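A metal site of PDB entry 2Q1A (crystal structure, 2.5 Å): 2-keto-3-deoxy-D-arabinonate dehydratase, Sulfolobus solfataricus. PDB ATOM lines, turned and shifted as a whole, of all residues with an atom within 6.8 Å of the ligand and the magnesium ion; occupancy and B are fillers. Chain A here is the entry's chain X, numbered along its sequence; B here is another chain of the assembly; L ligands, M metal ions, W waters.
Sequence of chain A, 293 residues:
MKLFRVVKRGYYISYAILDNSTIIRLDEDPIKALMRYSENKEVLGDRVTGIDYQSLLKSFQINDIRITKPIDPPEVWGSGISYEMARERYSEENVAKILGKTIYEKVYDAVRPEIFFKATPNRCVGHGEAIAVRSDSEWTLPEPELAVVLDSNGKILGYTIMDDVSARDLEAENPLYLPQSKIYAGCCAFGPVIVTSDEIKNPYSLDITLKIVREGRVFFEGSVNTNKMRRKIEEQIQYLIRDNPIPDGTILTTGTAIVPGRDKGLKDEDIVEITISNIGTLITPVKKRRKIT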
ATOM      1  N   GLY A  78       6.527  11.940 -24.307  1.00  0.00           N
ATOM      2  CA  GLY A  78       5.994  10.739 -24.925  1.00  0.00           C
ATOM      3  C   GLY A  78       5.803   9.584 -23.971  1.00  0.00           C
ATOM      4  O   GLY A  78       6.444   9.500 -22.915  1.00  0.00           O
ATOM      5  N   SER A  79       4.894   8.694 -24.339  1.00  0.00           N
ATOM      6  CA  SER A  79       4.683   7.456 -23.623  1.00  0.00           C
ATOM      7  C   SER A  79       5.000   6.311 -24.570  1.00  0.00           C
ATOM      8  O   SER A  79       4.780   6.432 -25.774  1.00  0.00           O
ATOM      9  CB  SER A  79       3.242   7.365 -23.152  1.00  0.00           C
ATOM     10  OG  SER A  79       3.151   6.630 -21.956  1.00  0.00           O
ATOM     11  N   GLY A  80       5.512   5.210 -24.047  1.00  0.00           N
ATOM     12  CA  GLY A  80       5.934   4.108 -24.894  1.00  0.00           C
ATOM     13  C   GLY A  80       5.257   2.779 -24.600  1.00  0.00           C
ATOM     14  O   GLY A  80       4.927   2.492 -23.452  1.00  0.00           O
ATOM     15  N   ILE A  81       5.068   1.992 -25.660  1.00  0.00           N
ATOM     16  CA  ILE A  81       4.558   0.612 -25.572  1.00  0.00           C
ATOM     17  C   ILE A  81       3.215   0.520 -24.836  1.00  0.00           C
ATOM     18  O   ILE A  81       3.085  -0.151 -23.808  1.00  0.00           O
ATOM     19  CB  ILE A  81       5.635  -0.351 -24.954  1.00  0.00           C
ATOM     20  CG1 ILE A  81       7.049  -0.030 -25.447  1.00  0.00           C
ATOM     21  CG2 ILE A  81       5.273  -1.825 -25.211  1.00  0.00           C
ATOM     22  CD1 ILE A  81       7.262  -0.155 -26.957  1.00  0.00           C
ATOM     23  N   SER A  82       2.207   1.200 -25.387  1.00  0.00           N
ATOM     24  CA  SER A  82       0.878   1.266 -24.761  1.00  0.00           C
ATOM     25  C   SER A  82      -0.193   0.458 -25.507  1.00  0.00           C
ATOM     26  O   SER A  82      -1.382   0.519 -25.164  1.00  0.00           O
ATOM     27  CB  SER A  82       0.448   2.725 -24.598  1.00  0.00           C
ATOM     28  OG  SER A  82       0.457   3.412 -25.837  1.00  0.00           O
ATOM     29  N   TYR A  83       0.235  -0.312 -26.509  1.00  0.00           N
ATOM     30  CA  TYR A  83      -0.657  -1.182 -27.269  1.00  0.00           C
ATOM     31  C   TYR A  83      -0.185  -2.635 -27.226  1.00  0.00           C
ATOM     32  O   TYR A  83       1.005  -2.888 -27.032  1.00  0.00           O
ATOM     33  CB  TYR A  83      -0.759  -0.713 -28.723  1.00  0.00           C
ATOM     34  CG  TYR A  83      -1.586   0.537 -28.932  1.00  0.00           C
ATOM     35  CD1 TYR A  83      -1.012   1.805 -28.794  1.00  0.00           C
ATOM     36  CD2 TYR A  83      -2.942   0.468 -29.276  1.00  0.00           C
ATOM     37  CE1 TYR A  83      -1.751   2.963 -28.987  1.00  0.00           C
ATOM     38  CE2 TYR A  83      -3.692   1.623 -29.477  1.00  0.00           C
ATOM     39  CZ  TYR A  83      -3.100   2.864 -29.331  1.00  0.00           C
ATOM     40  OH  TYR A  83      -3.835   4.002 -29.524  1.00  0.00           O
ATOM     41  N   ALA A  86       2.676  -3.681 -29.512  1.00  0.00           N
ATOM     42  CA  ALA A  86       3.892  -2.903 -29.255  1.00  0.00           C
ATOM     43  C   ALA A  86       5.003  -3.676 -28.517  1.00  0.00           C
ATOM     44  O   ALA A  86       6.159  -3.226 -28.502  1.00  0.00           O
ATOM     45  CB  ALA A  86       3.558  -1.584 -28.545  1.00  0.00           C
ATOM     46  N   ARG A  89       7.610  -4.346 -30.998  1.00  0.00           N
ATOM     47  CA  ARG A  89       8.379  -3.208 -31.518  1.00  0.00           C
ATOM     48  C   ARG A  89       9.856  -3.608 -31.562  1.00  0.00           C
ATOM     49  O   ARG A  89      10.542  -3.600 -30.538  1.00  0.00           O
ATOM     50  CB  ARG A  89       8.164  -1.957 -30.667  1.00  0.00           C
ATOM     51  CG  ARG A  89       8.886  -0.707 -31.181  1.00  0.00           C
ATOM     52  CD  ARG A  89       9.045   0.309 -30.062  1.00  0.00           C
ATOM     53  NE  ARG A  89       9.900   1.443 -30.426  1.00  0.00           N
ATOM     54  CZ  ARG A  89       9.451   2.619 -30.863  1.00  0.00           C
ATOM     55  NH1 ARG A  89       8.143   2.835 -31.011  1.00  0.00           N
ATOM     56  NH2 ARG A  89      10.308   3.589 -31.150  1.00  0.00           N
ATOM     57  N   TYR A 104      11.231  -3.997 -24.100  1.00  0.00           N
ATOM     58  CA  TYR A 104       9.893  -3.579 -24.514  1.00  0.00           C
ATOM     59  C   TYR A 104       8.837  -4.557 -23.992  1.00  0.00           C
ATOM     60  O   TYR A 104       7.749  -4.145 -23.579  1.00  0.00           O
ATOM     61  CB  TYR A 104       9.806  -3.464 -26.042  1.00  0.00           C
ATOM     62  CG  TYR A 104      10.892  -2.591 -26.639  1.00  0.00           C
ATOM     63  CD1 TYR A 104      10.781  -1.201 -26.630  1.00  0.00           C
ATOM     64  CD2 TYR A 104      12.033  -3.153 -27.211  1.00  0.00           C
ATOM     65  CE1 TYR A 104      11.770  -0.392 -27.164  1.00  0.00           C
ATOM     66  CE2 TYR A 104      13.034  -2.352 -27.747  1.00  0.00           C
ATOM     67  CZ  TYR A 104      12.896  -0.968 -27.723  1.00  0.00           C
ATOM     68  OH  TYR A 104      13.879  -0.171 -28.245  1.00  0.00           O
ATOM     69  N   GLU A 114       6.486   3.409 -19.633  1.00  0.00           N
ATOM     70  CA  GLU A 114       7.583   4.181 -20.188  1.00  0.00           C
ATOM     71  C   GLU A 114       7.124   5.619 -20.437  1.00  0.00           C
ATOM     72  O   GLU A 114       6.041   5.851 -20.989  1.00  0.00           O
ATOM     73  CB  GLU A 114       8.095   3.548 -21.487  1.00  0.00           C
ATOM     74  CG  GLU A 114       9.408   4.163 -21.989  1.00  0.00           C
ATOM     75  CD  GLU A 114       9.684   3.858 -23.445  1.00  0.00           C
ATOM     76  OE1 GLU A 114       8.959   3.013 -24.036  1.00  0.00           O
ATOM     77  OE2 GLU A 114      10.624   4.450 -24.003  1.00  0.00           O
ATOM     78  N   PHE A 116       9.157   9.354 -21.646  1.00  0.00           N
ATOM     79  CA  PHE A 116      10.394   9.992 -22.082  1.00  0.00           C
ATOM     80  C   PHE A 116      10.151  11.440 -22.488  1.00  0.00           C
ATOM     81  O   PHE A 116       9.006  11.828 -22.767  1.00  0.00           O
ATOM     82  CB  PHE A 116      11.056   9.216 -23.224  1.00  0.00           C
ATOM     83  CG  PHE A 116      10.182   9.065 -24.449  1.00  0.00           C
ATOM     84  CD1 PHE A 116      10.303   9.969 -25.514  1.00  0.00           C
ATOM     85  CD2 PHE A 116       9.247   8.041 -24.542  1.00  0.00           C
ATOM     86  CE1 PHE A 116       9.494   9.852 -26.642  1.00  0.00           C
ATOM     87  CE2 PHE A 116       8.421   7.910 -25.666  1.00  0.00           C
ATOM     88  CZ  PHE A 116       8.553   8.817 -26.723  1.00  0.00           C
ATOM     89  N   GLU A 143       5.351   8.006 -36.163  1.00  0.00           N
ATOM     90  CA  GLU A 143       4.500   7.294 -35.221  1.00  0.00           C
ATOM     91  C   GLU A 143       3.188   8.058 -34.988  1.00  0.00           C
ATOM     92  O   GLU A 143       3.164   9.068 -34.291  1.00  0.00           O
ATOM     93  CB  GLU A 143       5.252   7.006 -33.915  1.00  0.00           C
ATOM     94  CG  GLU A 143       6.452   6.063 -34.079  1.00  0.00           C
ATOM     95  CD  GLU A 143       7.093   5.636 -32.756  1.00  0.00           C
ATOM     96  OE1 GLU A 143       8.100   4.882 -32.784  1.00  0.00           O
ATOM     97  OE2 GLU A 143       6.604   6.062 -31.679  1.00  0.00           O
ATOM     98  N   GLU A 145      -0.012   9.087 -33.327  1.00  0.00           N
ATOM     99  CA  GLU A 145      -0.393   8.989 -31.919  1.00  0.00           C
ATOM    100  C   GLU A 145      -1.474  10.009 -31.547  1.00  0.00           C
ATOM    101  O   GLU A 145      -1.496  11.119 -32.069  1.00  0.00           O
ATOM    102  CB  GLU A 145       0.831   9.184 -31.021  1.00  0.00           C
ATOM    103  CG  GLU A 145       1.992   8.234 -31.329  1.00  0.00           C
ATOM    104  CD  GLU A 145       3.083   8.242 -30.276  1.00  0.00           C
ATOM    105  OE1 GLU A 145       4.153   7.640 -30.536  1.00  0.00           O
ATOM    106  OE2 GLU A 145       2.887   8.818 -29.182  1.00  0.00           O
ATOM    107  N   ASP A 164       5.141  11.233 -33.518  1.00  0.00           N
ATOM    108  CA  ASP A 164       6.380  10.973 -32.803  1.00  0.00           C
ATOM    109  C   ASP A 164       7.444  10.430 -33.768  1.00  0.00           C
ATOM    110  O   ASP A 164       7.711   9.220 -33.835  1.00  0.00           O
ATOM    111  CB  ASP A 164       6.119  10.044 -31.586  1.00  0.00           C
ATOM    112  CG  ASP A 164       7.401   9.578 -30.893  1.00  0.00           C
ATOM    113  OD1 ASP A 164       8.446  10.249 -30.965  1.00  0.00           O
ATOM    114  OD2 ASP A 164       7.365   8.504 -30.259  1.00  0.00           O
ATOM    115  N   VAL A 165       8.062  11.331 -34.516  1.00  0.00           N
ATOM    116  CA  VAL A 165       9.080  10.963 -35.508  1.00  0.00           C
ATOM    117  C   VAL A 165      10.274  10.282 -34.821  1.00  0.00           C
ATOM    118  O   VAL A 165      10.878  10.849 -33.921  1.00  0.00           O
ATOM    119  CB  VAL A 165       9.516  12.193 -36.361  1.00  0.00           C
ATOM    120  CG1 VAL A 165      10.374  11.770 -37.523  1.00  0.00           C
ATOM    121  CG2 VAL A 165       8.292  12.946 -36.861  1.00  0.00           C
ATOM    122  N   SER A 166      10.602   9.061 -35.257  1.00  0.00           N
ATOM    123  CA  SER A 166      11.642   8.263 -34.585  1.00  0.00           C
ATOM    124  C   SER A 166      12.697   7.677 -35.537  1.00  0.00           C
ATOM    125  O   SER A 166      12.362   6.957 -36.477  1.00  0.00           O
ATOM    126  CB  SER A 166      10.997   7.119 -33.784  1.00  0.00           C
ATOM    127  OG  SER A 166       9.855   7.545 -33.064  1.00  0.00           O
ATOM    128  N   GLU A 171      17.763   3.669 -32.286  1.00  0.00           N
ATOM    129  CA  GLU A 171      17.186   3.018 -31.116  1.00  0.00           C
ATOM    130  C   GLU A 171      17.540   1.528 -31.079  1.00  0.00           C
ATOM    131  O   GLU A 171      17.847   0.988 -30.021  1.00  0.00           O
ATOM    132  CB  GLU A 171      15.667   3.204 -31.108  1.00  0.00           C
ATOM    133  CG  GLU A 171      14.920   2.310 -30.120  1.00  0.00           C
ATOM    134  CD  GLU A 171      13.419   2.410 -30.267  1.00  0.00           C
ATOM    135  OE1 GLU A 171      12.940   3.246 -31.074  1.00  0.00           O
ATOM    136  OE2 GLU A 171      12.701   1.672 -29.565  1.00  0.00           O
ATOM    137  N   LEU A 178      18.242   6.234 -27.555  1.00  0.00           N
ATOM    138  CA  LEU A 178      16.849   6.666 -27.672  1.00  0.00           C
ATOM    139  C   LEU A 178      16.631   8.197 -27.718  1.00  0.00           C
ATOM    140  O   LEU A 178      15.896   8.677 -28.584  1.00  0.00           O
ATOM    141  CB  LEU A 178      15.997   5.984 -26.598  1.00  0.00           C
ATOM    142  CG  LEU A 178      14.486   5.743 -26.773  1.00  0.00           C
ATOM    143  CD1 LEU A 178      14.098   5.213 -28.147  1.00  0.00           C
ATOM    144  CD2 LEU A 178      14.005   4.776 -25.694  1.00  0.00           C
ATOM    145  N   LYS A 182      15.036  10.474 -30.877  1.00  0.00           N
ATOM    146  CA  LYS A 182      13.724  11.083 -30.618  1.00  0.00           C
ATOM    147  C   LYS A 182      13.685  12.613 -30.609  1.00  0.00           C
ATOM    148  O   LYS A 182      12.632  13.206 -30.872  1.00  0.00           O
ATOM    149  CB  LYS A 182      13.139  10.550 -29.307  1.00  0.00           C
ATOM    150  CG  LYS A 182      12.709   9.088 -29.326  1.00  0.00           C
ATOM    151  CD  LYS A 182      11.261   8.926 -29.709  1.00  0.00           C
ATOM    152  CE  LYS A 182      10.873   7.464 -29.828  1.00  0.00           C
ATOM    153  NZ  LYS A 182       9.430   7.272 -30.171  1.00  0.00           N
ATOM    154  N   THR A 253       2.057  12.721 -25.605  1.00  0.00           N
ATOM    155  CA  THR A 253       1.687  11.831 -26.696  1.00  0.00           C
ATOM    156  C   THR A 253       1.664  10.373 -26.225  1.00  0.00           C
ATOM    157  O   THR A 253       2.628   9.877 -25.630  1.00  0.00           O
ATOM    158  CB  THR A 253       2.547  12.067 -27.972  1.00  0.00           C
ATOM    159  OG1 THR A 253       2.017  11.295 -29.043  1.00  0.00           O
ATOM    160  CG2 THR A 253       4.016  11.713 -27.759  1.00  0.00           C
ATOM    161  N   THR A 254       0.551   9.691 -26.487  1.00  0.00           N
ATOM    162  CA  THR A 254       0.181   8.457 -25.770  1.00  0.00           C
ATOM    163  C   THR A 254       0.693   7.115 -26.311  1.00  0.00           C
ATOM    164  O   THR A 254       0.274   6.058 -25.834  1.00  0.00           O
ATOM    165  CB  THR A 254      -1.337   8.373 -25.559  1.00  0.00           C
ATOM    166  OG1 THR A 254      -1.997   8.251 -26.830  1.00  0.00           O
ATOM    167  CG2 THR A 254      -1.852   9.620 -24.841  1.00  0.00           C
ATOM    168  N   GLY A 255       1.589   7.139 -27.301  1.00  0.00           N
ATOM    169  CA  GLY A 255       2.133   5.897 -27.872  1.00  0.00           C
ATOM    170  C   GLY A 255       1.447   5.462 -29.168  1.00  0.00           C
ATOM    171  O   GLY A 255       0.265   5.748 -29.386  1.00  0.00           O
ATOM    172  N   THR A 256       2.183   4.760 -30.021  1.00  0.00           N
ATOM    173  CA  THR A 256       1.672   4.324 -31.332  1.00  0.00           C
ATOM    174  C   THR A 256       1.317   2.838 -31.416  1.00  0.00           C
ATOM    175  O   THR A 256       1.856   2.007 -30.672  1.00  0.00           O
ATOM    176  CB  THR A 256       2.633   4.683 -32.489  1.00  0.00           C
ATOM    177  OG1 THR A 256       1.942   4.584 -33.734  1.00  0.00           O
ATOM    178  CG2 THR A 256       3.859   3.764 -32.506  1.00  0.00           C
ATOM    179  N   ALA A 257       0.423   2.513 -32.336  1.00  0.00           N
ATOM    180  CA  ALA A 257       0.063   1.122 -32.636  1.00  0.00           C
ATOM    181  C   ALA A 257       0.369   0.741 -34.086  1.00  0.00           C
ATOM    182  O   ALA A 257       0.303  -0.438 -34.453  1.00  0.00           O
ATOM    183  CB  ALA A 257      -1.399   0.876 -32.340  1.00  0.00           C
ATOM    184  N   LEU B 176      14.637   1.699 -19.985  1.00  0.00           N
ATOM    185  CA  LEU B 176      13.572   2.540 -20.530  1.00  0.00           C
ATOM    186  C   LEU B 176      13.028   3.519 -19.501  1.00  0.00           C
ATOM    187  O   LEU B 176      12.292   4.443 -19.840  1.00  0.00           O
ATOM    188  CB  LEU B 176      12.433   1.683 -21.107  1.00  0.00           C
ATOM    189  CG  LEU B 176      12.738   0.878 -22.379  1.00  0.00           C
ATOM    190  CD1 LEU B 176      11.491   0.160 -22.919  1.00  0.00           C
ATOM    191  CD2 LEU B 176      13.364   1.755 -23.464  1.00  0.00           C
HETATM  192  C1  LIG L   1       9.130   4.256 -27.858  1.00  0.00           C
HETATM  193  C2  LIG L   1       7.912   3.813 -27.861  1.00  0.00           C
HETATM  194  C3  LIG L   1       7.078   4.575 -28.440  1.00  0.00           C
HETATM  195  O1  LIG L   1       7.411   5.693 -28.861  1.00  0.00           O
HETATM  196  C4  LIG L   1       5.812   4.175 -28.618  1.00  0.00           C
HETATM  197  O2  LIG L   1       5.447   3.049 -28.211  1.00  0.00           O
HETATM  198  O3  LIG L   1       5.010   4.933 -29.204  1.00  0.00           O
HETATM  199 MG    MG M   1       6.009   6.999 -29.944  1.00  0.00          MG
HETATM  200  O   HOH W   1       2.952   2.303 -28.138  1.00  0.00           O
HETATM  201  O   HOH W   2       5.108   7.751 -28.079  1.00  0.00           O
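An oxygen (O2) of the ligand lies within hydrogen-bond range of the backbone NH (N) of Ile 81, 2.8 Å away.
O1 of the ligand sits close to NZ of Lys 182, at 2.9 Å.
N of Thr 256 sits close to O3 of the ligand, at 2.9 Å.
The guanidinium group (NH1) of Arg 89 is in salt-bridge range of an oxygen (O2) of the ligand (3.9 Å).
N of Gly 255 is in hydrogen-bond range of OE2 of Glu 145 (2.8 Å).
The side-chain hydroxyl (OG1) of Thr 253 sits at hydrogen-bond distance from the side-chain carboxylate (OE2) of Glu 145 (2.6 Å).
The side-chain carboxylate of Glu 143 is in salt-bridge range of the side-chain amino group of Lys 182 (3.8 Å).
The side-chain amino group of Lys 182 is in hydrogen-bond range of the side-chain hydroxyl of Ser 166 (2.9 Å).
O of Glu 114 lies within hydrogen-bond range of N of Gly 80 (3.2 Å).
The side-chain hydroxyl of Ser 79 is in hydrogen-bond range of the backbone carbonyl oxygen of Glu 114, at 3.1 Å.
The backbone carbonyl oxygen of Thr 253 is in hydrogen-bond range of the backbone NH of Ser 79.
N of Gly 78 lies within hydrogen-bond range of O of Phe 116 (2.9 Å).
Ser 79 touches the ligand (O to O3, 3.8 Å).
Gly 80 touches the ligand.
Phe 116 touches the ligand.
CA of Gly 255 touches O3 of the ligand, at 3.3 Å.
Hydrophobic or aromatic side chains within 4 Å of the ligand: Ile 81 and Phe 116.
Of the 25 residues printed, 11 come within 4 Å of the ligand.
Along chain A the residues within 4 Å of the ligand span positions 79 to 256.
The nearest printed residue that does not touch the ligand is Glu 114 (4.02 Å).
Merely in contact with the magnesium ion: Lys 182.
Within 4 Å of the magnesium ion: Glu 143, Glu 145, Asp 164 and Lys 182.
The nearest printed residue that does not touch the magnesium ion is Ser 79 (4.4 Å).
The magnesium ion is bound by the side-chain carboxylate (OD2) of Asp 164 (2.1 Å).
The magnesium ion is bound by the side-chain carboxylate (OE1) of Glu 145, 2.1 Å away.
OE2 of Glu 143 is bound to the magnesium ion (2.1 Å).
An oxygen (O1) of the ligand is bound to the magnesium ion (2.2 Å).
Water W2 is bound to the magnesium ion (2.2 Å).
O3 of the ligand is bound to the magnesium ion (2.4 Å).
The magnesium ion has six donor atoms within binding distance.
Water W2 bridges O of Ser 79 (2.7 Å) and OE2 of Glu 145 (2.7 Å).
Water W1 lies within hydrogen-bond range of O2 of the ligand, O of Thr 256, N of Ser 82 and N of Ile 81.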
